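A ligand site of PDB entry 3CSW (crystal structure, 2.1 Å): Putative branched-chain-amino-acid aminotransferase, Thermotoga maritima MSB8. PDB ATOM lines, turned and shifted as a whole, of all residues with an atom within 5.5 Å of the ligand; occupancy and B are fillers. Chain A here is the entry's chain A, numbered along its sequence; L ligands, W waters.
The backbone carbonyl oxygen (O) of His 239 sits close to the side-chain hydroxyl (OG1) of Thr 204 (3.4 Å).
OE2 of Glu 176 lies within salt-bridge range of NE of Arg 134 (2.7 Å).
The backbone carbonyl oxygen of Asp 201 is in hydrogen-bond range of the guanidinium group of Arg 62 (3.2 Å).
O of Lys 145 is in hydrogen-bond range of N of Tyr 43 (3.0 Å).
The guanidinium group (NH2) of Arg 156 sits at hydrogen-bond distance from the backbone carbonyl oxygen (O) of Ser 178 (2.9 Å).
The backbone NH of Gly 202 lies close to the side-chain amide oxygen of Asn 181 (3.4 Å).
O of Leu 200 is in hydrogen-bond range of ND2 of Asn 181 (3.2 Å).
N of Thr 238 is in hydrogen-bond range of O of Asn 181, at 2.9 Å.
The backbone NH (N) of Thr 204 lies close to an oxygen (O5) of the ligand, 3.0 Å away.
OG1 of Thr 204 lies close to O5 of the ligand (2.7 Å).
The side-chain carboxylate of Glu 176 sits close to a nitrogen (N1) of the ligand, at 2.8 Å.
An oxygen (O6) of the ligand sits close to the backbone NH (N) of Thr 240.
An oxygen (O6) of the ligand lies close to the side-chain hydroxyl of Thr 240.
N of Ile 203 sits close to O4 of the ligand.
The guanidinium group of Arg 62 lies close to an oxygen (O4) of the ligand, at 2.9 Å.
The backbone carbonyl oxygen of Phe 179 sits close to an oxygen (O2) of the ligand (3.1 Å).
The guanidinium group (NH2) of Arg 156 sits close to an oxygen (O1) of the ligand (3.3 Å).
Water W1 lies within hydrogen-bond range of OD1 of Asn 181 (2.7 Å), OG1 of Thr 238 (2.8 Å) and N of Arg 205 (3.0 Å).
Water W4 lies within hydrogen-bond range of OG1 of Thr 45 (2.7 Å), NH2 of Arg 62 (3.1 Å) and OG1 of Thr 240 (3.3 Å).
Water W3 lies within hydrogen-bond range of OG1 of Thr 45 (2.6 Å) and NZ of Lys 145 (2.8 Å).
NZ of Lys 145 touches C5 of the ligand (3.0 Å).
Ile 152 touches the ligand (CD1 to C2, 3.5 Å).
Gly 177 touches the ligand.
O of Ser 178 touches C2 of the ligand, at 3.5 Å.
Ser 180 touches the ligand (C to C7, 3.4 Å).
OD1 of Asn 181 touches C7 of the ligand (3.6 Å).
Leu 200 touches the ligand.
Gly 202 touches the ligand (CA to O3, 3.5 Å).
His 239 touches the ligand (CA to O5, 3.9 Å).
Hydrophobic or aromatic side chains that line the ligand: Ile 152, Leu 200 and Ile 203.
Within 4 Å of the ligand: Arg 62, Lys 145, Ile 152, Arg 156, Glu 176, Gly 177, Ser 178, Phe 179, Ser 180, Asn 181, Leu 200, Gly 202, Ile 203, Thr 204, His 239 and Thr 240.
Along chain A the residues within 4 Å of the ligand span positions 62 to 240.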
ATOM      1  N   TYR A  43      27.145  14.124  11.246  1.00  0.00           N
ATOM      2  CA  TYR A  43      28.225  14.097  12.220  1.00  0.00           C
ATOM      3  C   TYR A  43      27.878  13.662  13.644  1.00  0.00           C
ATOM      4  O   TYR A  43      26.712  13.655  14.039  1.00  0.00           O
ATOM      5  CB  TYR A  43      28.895  15.480  12.273  1.00  0.00           C
ATOM      6  CG  TYR A  43      28.141  16.513  13.088  1.00  0.00           C
ATOM      7  CD1 TYR A  43      27.093  17.228  12.518  1.00  0.00           C
ATOM      8  CD2 TYR A  43      28.491  16.786  14.415  1.00  0.00           C
ATOM      9  CE1 TYR A  43      26.398  18.184  13.249  1.00  0.00           C
ATOM     10  CE2 TYR A  43      27.804  17.744  15.151  1.00  0.00           C
ATOM     11  CZ  TYR A  43      26.758  18.426  14.556  1.00  0.00           C
ATOM     12  OH  TYR A  43      26.051  19.373  15.238  1.00  0.00           O
ATOM     13  N   THR A  45      29.891  13.841  17.838  1.00  0.00           N
ATOM     14  CA  THR A  45      30.979  14.329  18.699  1.00  0.00           C
ATOM     15  C   THR A  45      31.123  13.374  19.879  1.00  0.00           C
ATOM     16  O   THR A  45      30.136  12.917  20.424  1.00  0.00           O
ATOM     17  CB  THR A  45      30.749  15.768  19.214  1.00  0.00           C
ATOM     18  OG1 THR A  45      29.604  15.826  20.071  1.00  0.00           O
ATOM     19  CG2 THR A  45      30.579  16.748  18.043  1.00  0.00           C
ATOM     20  N   HIS A  59      27.042   6.490  19.882  1.00  0.00           N
ATOM     21  CA  HIS A  59      27.329   7.496  18.860  1.00  0.00           C
ATOM     22  C   HIS A  59      27.350   6.906  17.461  1.00  0.00           C
ATOM     23  O   HIS A  59      26.881   7.526  16.530  1.00  0.00           O
ATOM     24  CB  HIS A  59      28.648   8.198  19.165  1.00  0.00           C
ATOM     25  CG  HIS A  59      28.532   9.224  20.242  1.00  0.00           C
ATOM     26  ND1 HIS A  59      27.956  10.457  20.030  1.00  0.00           N
ATOM     27  CD2 HIS A  59      28.918   9.205  21.543  1.00  0.00           C
ATOM     28  CE1 HIS A  59      27.986  11.151  21.152  1.00  0.00           C
ATOM     29  NE2 HIS A  59      28.577  10.429  22.079  1.00  0.00           N
ATOM     30  N   ARG A  62      23.734   6.420  16.283  1.00  0.00           N
ATOM     31  CA  ARG A  62      23.124   7.726  15.954  1.00  0.00           C
ATOM     32  C   ARG A  62      23.623   8.198  14.605  1.00  0.00           C
ATOM     33  O   ARG A  62      22.875   8.783  13.837  1.00  0.00           O
ATOM     34  CB  ARG A  62      23.469   8.819  16.988  1.00  0.00           C
ATOM     35  CG  ARG A  62      22.356   9.197  17.974  1.00  0.00           C
ATOM     36  CD  ARG A  62      22.278  10.734  18.149  1.00  0.00           C
ATOM     37  NE  ARG A  62      23.541  11.325  18.604  1.00  0.00           N
ATOM     38  CZ  ARG A  62      23.671  12.179  19.620  1.00  0.00           C
ATOM     39  NH1 ARG A  62      22.632  12.584  20.327  1.00  0.00           N
ATOM     40  NH2 ARG A  62      24.875  12.628  19.932  1.00  0.00           N
ATOM     41  N   ARG A 134      13.319  25.989  16.809  1.00  0.00           N
ATOM     42  CA  ARG A 134      13.701  24.675  16.320  1.00  0.00           C
ATOM     43  C   ARG A 134      12.843  24.291  15.113  1.00  0.00           C
ATOM     44  O   ARG A 134      11.627  24.494  15.141  1.00  0.00           O
ATOM     45  CB  ARG A 134      13.536  23.651  17.441  1.00  0.00           C
ATOM     46  CG  ARG A 134      14.196  22.297  17.194  1.00  0.00           C
ATOM     47  CD  ARG A 134      15.674  22.402  17.471  1.00  0.00           C
ATOM     48  NE  ARG A 134      16.294  21.102  17.681  1.00  0.00           N
ATOM     49  CZ  ARG A 134      17.129  20.479  16.848  1.00  0.00           C
ATOM     50  NH1 ARG A 134      17.470  20.994  15.677  1.00  0.00           N
ATOM     51  NH2 ARG A 134      17.644  19.306  17.204  1.00  0.00           N
ATOM     52  N   LYS A 145      21.488  15.016  12.608  1.00  0.00           N
ATOM     53  CA  LYS A 145      22.663  15.814  12.984  1.00  0.00           C
ATOM     54  C   LYS A 145      23.490  16.037  11.732  1.00  0.00           C
ATOM     55  O   LYS A 145      24.289  15.168  11.360  1.00  0.00           O
ATOM     56  CB  LYS A 145      23.547  15.106  13.992  1.00  0.00           C
ATOM     57  CG  LYS A 145      23.150  15.231  15.414  1.00  0.00           C
ATOM     58  CD  LYS A 145      24.135  14.480  16.319  1.00  0.00           C
ATOM     59  CE  LYS A 145      25.296  15.316  16.736  1.00  0.00           C
ATOM     60  NZ  LYS A 145      25.036  15.968  18.055  1.00  0.00           N
ATOM     61  N   ILE A 152      20.296  25.265  14.036  1.00  0.00           N
ATOM     62  CA  ILE A 152      21.504  25.127  14.848  1.00  0.00           C
ATOM     63  C   ILE A 152      22.619  26.073  14.347  1.00  0.00           C
ATOM     64  O   ILE A 152      23.287  26.726  15.163  1.00  0.00           O
ATOM     65  CB  ILE A 152      21.998  23.649  14.899  1.00  0.00           C
ATOM     66  CG1 ILE A 152      20.928  22.716  15.489  1.00  0.00           C
ATOM     67  CG2 ILE A 152      23.312  23.567  15.668  1.00  0.00           C
ATOM     68  CD1 ILE A 152      20.348  23.121  16.898  1.00  0.00           C
ATOM     69  N   ARG A 156      23.718  29.048  17.016  1.00  0.00           N
ATOM     70  CA  ARG A 156      25.080  29.102  17.534  1.00  0.00           C
ATOM     71  C   ARG A 156      25.760  30.438  17.283  1.00  0.00           C
ATOM     72  O   ARG A 156      26.600  30.836  18.065  1.00  0.00           O
ATOM     73  CB  ARG A 156      25.951  27.982  16.969  1.00  0.00           C
ATOM     74  CG  ARG A 156      25.486  26.663  17.440  1.00  0.00           C
ATOM     75  CD  ARG A 156      26.542  25.640  17.481  1.00  0.00           C
ATOM     76  NE  ARG A 156      25.959  24.373  17.884  1.00  0.00           N
ATOM     77  CZ  ARG A 156      26.477  23.185  17.611  1.00  0.00           C
ATOM     78  NH1 ARG A 156      27.626  23.083  16.970  1.00  0.00           N
ATOM     79  NH2 ARG A 156      25.845  22.080  17.987  1.00  0.00           N
ATOM     80  N   GLU A 176      15.653  22.595  23.244  1.00  0.00           N
ATOM     81  CA  GLU A 176      16.976  22.337  23.707  1.00  0.00           C
ATOM     82  C   GLU A 176      17.899  23.506  23.431  1.00  0.00           C
ATOM     83  O   GLU A 176      17.524  24.441  22.754  1.00  0.00           O
ATOM     84  CB  GLU A 176      17.511  21.079  22.992  1.00  0.00           C
ATOM     85  CG  GLU A 176      17.587  21.192  21.469  1.00  0.00           C
ATOM     86  CD  GLU A 176      17.570  19.847  20.771  1.00  0.00           C
ATOM     87  OE1 GLU A 176      18.406  18.981  21.082  1.00  0.00           O
ATOM     88  OE2 GLU A 176      16.705  19.650  19.898  1.00  0.00           O
ATOM     89  N   GLY A 177      19.125  23.440  23.937  1.00  0.00           N
ATOM     90  CA  GLY A 177      20.154  24.396  23.565  1.00  0.00           C
ATOM     91  C   GLY A 177      20.692  24.087  22.176  1.00  0.00           C
ATOM     92  O   GLY A 177      20.438  23.019  21.642  1.00  0.00           O
ATOM     93  N   SER A 178      21.472  25.021  21.597  1.00  0.00           N
ATOM     94  CA  SER A 178      22.117  24.842  20.274  1.00  0.00           C
ATOM     95  C   SER A 178      23.120  23.674  20.217  1.00  0.00           C
ATOM     96  O   SER A 178      23.410  23.140  19.139  1.00  0.00           O
ATOM     97  CB  SER A 178      22.758  26.157  19.776  1.00  0.00           C
ATOM     98  OG  SER A 178      23.993  26.469  20.422  1.00  0.00           O
ATOM     99  N   PHE A 179      23.645  23.261  21.374  1.00  0.00           N
ATOM    100  CA  PHE A 179      24.599  22.146  21.448  1.00  0.00           C
ATOM    101  C   PHE A 179      24.425  21.292  22.725  1.00  0.00           C
ATOM    102  O   PHE A 179      25.309  20.494  23.049  1.00  0.00           O
ATOM    103  CB  PHE A 179      26.057  22.645  21.334  1.00  0.00           C
ATOM    104  CG  PHE A 179      26.524  23.563  22.476  1.00  0.00           C
ATOM    105  CD1 PHE A 179      27.032  23.039  23.678  1.00  0.00           C
ATOM    106  CD2 PHE A 179      26.498  24.957  22.325  1.00  0.00           C
ATOM    107  CE1 PHE A 179      27.454  23.888  24.700  1.00  0.00           C
ATOM    108  CE2 PHE A 179      26.942  25.807  23.351  1.00  0.00           C
ATOM    109  CZ  PHE A 179      27.406  25.262  24.551  1.00  0.00           C
ATOM    110  N   SER A 180      23.282  21.434  23.411  1.00  0.00           N
ATOM    111  CA  SER A 180      23.024  20.747  24.671  1.00  0.00           C
ATOM    112  C   SER A 180      21.549  20.457  24.848  1.00  0.00           C
ATOM    113  O   SER A 180      20.746  21.037  24.172  1.00  0.00           O
ATOM    114  CB  SER A 180      23.470  21.637  25.849  1.00  0.00           C
ATOM    115  OG  SER A 180      22.818  22.911  25.844  1.00  0.00           O
ATOM    116  N   ASN A 181      21.201  19.540  25.766  1.00  0.00           N
ATOM    117  CA  ASN A 181      19.824  19.366  26.215  1.00  0.00           C
ATOM    118  C   ASN A 181      19.586  20.134  27.532  1.00  0.00           C
ATOM    119  O   ASN A 181      20.523  20.484  28.252  1.00  0.00           O
ATOM    120  CB  ASN A 181      19.460  17.896  26.367  1.00  0.00           C
ATOM    121  CG  ASN A 181      19.393  17.162  25.035  1.00  0.00           C
ATOM    122  OD1 ASN A 181      20.273  16.348  24.724  1.00  0.00           O
ATOM    123  ND2 ASN A 181      18.339  17.424  24.248  1.00  0.00           N
ATOM    124  N   LEU A 200      16.750  16.499  19.777  1.00  0.00           N
ATOM    125  CA  LEU A 200      17.791  15.484  19.648  1.00  0.00           C
ATOM    126  C   LEU A 200      17.898  14.664  20.947  1.00  0.00           C
ATOM    127  O   LEU A 200      17.874  15.228  22.035  1.00  0.00           O
ATOM    128  CB  LEU A 200      19.097  16.173  19.379  1.00  0.00           C
ATOM    129  CG  LEU A 200      20.223  15.343  18.829  1.00  0.00           C
ATOM    130  CD1 LEU A 200      19.882  14.837  17.456  1.00  0.00           C
ATOM    131  CD2 LEU A 200      21.455  16.199  18.786  1.00  0.00           C
ATOM    132  N   ASP A 201      17.945  13.343  20.822  1.00  0.00           N
ATOM    133  CA  ASP A 201      18.067  12.418  21.969  1.00  0.00           C
ATOM    134  C   ASP A 201      19.539  12.334  22.391  1.00  0.00           C
ATOM    135  O   ASP A 201      20.252  11.396  22.056  1.00  0.00           O
ATOM    136  CB  ASP A 201      17.505  11.011  21.645  1.00  0.00           C
ATOM    137  CG  ASP A 201      18.048  10.431  20.332  1.00  0.00           C
ATOM    138  OD1 ASP A 201      18.408  11.217  19.411  1.00  0.00           O
ATOM    139  OD2 ASP A 201      18.107   9.196  20.209  1.00  0.00           O
ATOM    140  N   GLY A 202      19.985  13.358  23.095  1.00  0.00           N
ATOM    141  CA  GLY A 202      21.354  13.403  23.540  1.00  0.00           C
ATOM    142  C   GLY A 202      21.741  12.228  24.425  1.00  0.00           C
ATOM    143  O   GLY A 202      20.935  11.748  25.248  1.00  0.00           O
ATOM    144  N   ILE A 203      22.958  11.759  24.219  1.00  0.00           N
ATOM    145  CA  ILE A 203      23.538  10.653  24.992  1.00  0.00           C
ATOM    146  C   ILE A 203      23.833  11.060  26.464  1.00  0.00           C
ATOM    147  O   ILE A 203      23.707  10.211  27.351  1.00  0.00           O
ATOM    148  CB  ILE A 203      24.803  10.105  24.292  1.00  0.00           C
ATOM    149  CG1 ILE A 203      24.358   9.441  22.978  1.00  0.00           C
ATOM    150  CG2 ILE A 203      25.618   9.155  25.258  1.00  0.00           C
ATOM    151  CD1 ILE A 203      25.453   9.039  22.041  1.00  0.00           C
ATOM    152  N   THR A 204      24.199  12.313  26.712  1.00  0.00           N
ATOM    153  CA  THR A 204      24.364  12.819  28.099  1.00  0.00           C
ATOM    154  C   THR A 204      23.013  12.882  28.819  1.00  0.00           C
ATOM    155  O   THR A 204      22.874  12.467  29.956  1.00  0.00           O
ATOM    156  CB  THR A 204      25.035  14.216  28.161  1.00  0.00           C
ATOM    157  OG1 THR A 204      26.080  14.301  27.198  1.00  0.00           O
ATOM    158  CG2 THR A 204      25.594  14.518  29.574  1.00  0.00           C
ATOM    159  N   ARG A 205      22.028  13.427  28.125  1.00  0.00           N
ATOM    160  CA  ARG A 205      20.643  13.447  28.598  1.00  0.00           C
ATOM    161  C   ARG A 205      20.158  12.067  29.049  1.00  0.00           C
ATOM    162  O   ARG A 205      19.624  11.916  30.122  1.00  0.00           O
ATOM    163  CB  ARG A 205      19.758  13.996  27.461  1.00  0.00           C
ATOM    164  CG  ARG A 205      18.249  13.900  27.666  1.00  0.00           C
ATOM    165  CD  ARG A 205      17.521  14.143  26.364  1.00  0.00           C
ATOM    166  NE  ARG A 205      16.084  14.187  26.573  1.00  0.00           N
ATOM    167  CZ  ARG A 205      15.293  13.111  26.605  1.00  0.00           C
ATOM    168  NH1 ARG A 205      15.796  11.901  26.411  1.00  0.00           N
ATOM    169  NH2 ARG A 205      13.998  13.267  26.807  1.00  0.00           N
ATOM    170  N   THR A 238      23.020  19.593  29.498  1.00  0.00           N
ATOM    171  CA  THR A 238      23.825  18.390  29.341  1.00  0.00           C
ATOM    172  C   THR A 238      24.389  18.314  27.918  1.00  0.00           C
ATOM    173  O   THR A 238      23.683  18.505  26.948  1.00  0.00           O
ATOM    174  CB  THR A 238      22.982  17.089  29.644  1.00  0.00           C
ATOM    175  OG1 THR A 238      21.921  16.950  28.687  1.00  0.00           O
ATOM    176  CG2 THR A 238      22.370  17.134  31.039  1.00  0.00           C
ATOM    177  N   HIS A 239      25.684  18.038  27.795  1.00  0.00           N
ATOM    178  CA  HIS A 239      26.298  17.782  26.491  1.00  0.00           C
ATOM    179  C   HIS A 239      27.586  16.975  26.655  1.00  0.00           C
ATOM    180  O   HIS A 239      28.161  16.930  27.713  1.00  0.00           O
ATOM    181  CB  HIS A 239      26.532  19.091  25.684  1.00  0.00           C
ATOM    182  CG  HIS A 239      27.453  20.079  26.330  1.00  0.00           C
ATOM    183  ND1 HIS A 239      28.763  20.249  25.921  1.00  0.00           N
ATOM    184  CD2 HIS A 239      27.249  20.970  27.333  1.00  0.00           C
ATOM    185  CE1 HIS A 239      29.327  21.203  26.646  1.00  0.00           C
ATOM    186  NE2 HIS A 239      28.435  21.649  27.518  1.00  0.00           N
ATOM    187  N   THR A 240      28.025  16.327  25.573  1.00  0.00           N
ATOM    188  CA  THR A 240      29.144  15.391  25.617  1.00  0.00           C
ATOM    189  C   THR A 240      30.398  15.903  26.334  1.00  0.00           C
ATOM    190  O   THR A 240      30.932  15.216  27.238  1.00  0.00           O
ATOM    191  CB  THR A 240      29.531  14.911  24.169  1.00  0.00           C
ATOM    192  OG1 THR A 240      28.542  13.976  23.679  1.00  0.00           O
ATOM    193  CG2 THR A 240      30.862  14.215  24.184  1.00  0.00           C
HETATM  194  N1  LIG L   1      21.163  19.227  21.173  1.00  0.00           N
HETATM  195  C1  LIG L   1      21.829  19.583  20.003  1.00  0.00           C
HETATM  196  C2  LIG L   1      21.119  20.491  19.048  1.00  0.00           C
HETATM  197  C3  LIG L   1      23.127  19.099  19.763  1.00  0.00           C
HETATM  198  O1  LIG L   1      23.845  19.511  18.656  1.00  0.00           O
HETATM  199  C4  LIG L   1      23.747  18.246  20.714  1.00  0.00           C
HETATM  200  C5  LIG L   1      25.157  17.764  20.513  1.00  0.00           C
HETATM  201  O2  LIG L   1      26.116  18.490  20.830  1.00  0.00           O
HETATM  202  C6  LIG L   1      23.054  17.901  21.883  1.00  0.00           C
HETATM  203  C7  LIG L   1      21.761  18.395  22.096  1.00  0.00           C
HETATM  204  C8  LIG L   1      23.737  17.186  23.025  1.00  0.00           C
HETATM  205  O3  LIG L   1      23.761  15.788  22.788  1.00  0.00           O
HETATM  206  P1  LIG L   1      24.885  14.803  23.440  1.00  0.00           P
HETATM  207  O4  LIG L   1      24.817  13.422  22.755  1.00  0.00           O
HETATM  208  O5  LIG L   1      24.609  14.641  24.907  1.00  0.00           O
HETATM  209  O6  LIG L   1      26.216  15.494  23.205  1.00  0.00           O
HETATM  210  O   HOH W   1      22.479  15.687  26.204  1.00  0.00           O
HETATM  211  O   HOH W   2      27.724  19.498  18.438  1.00  0.00           O
HETATM  212  O   HOH W   3      27.626  16.767  18.712  1.00  0.00           O
HETATM  213  O   HOH W   4      27.424  14.319  20.609  1.00  0.00           O
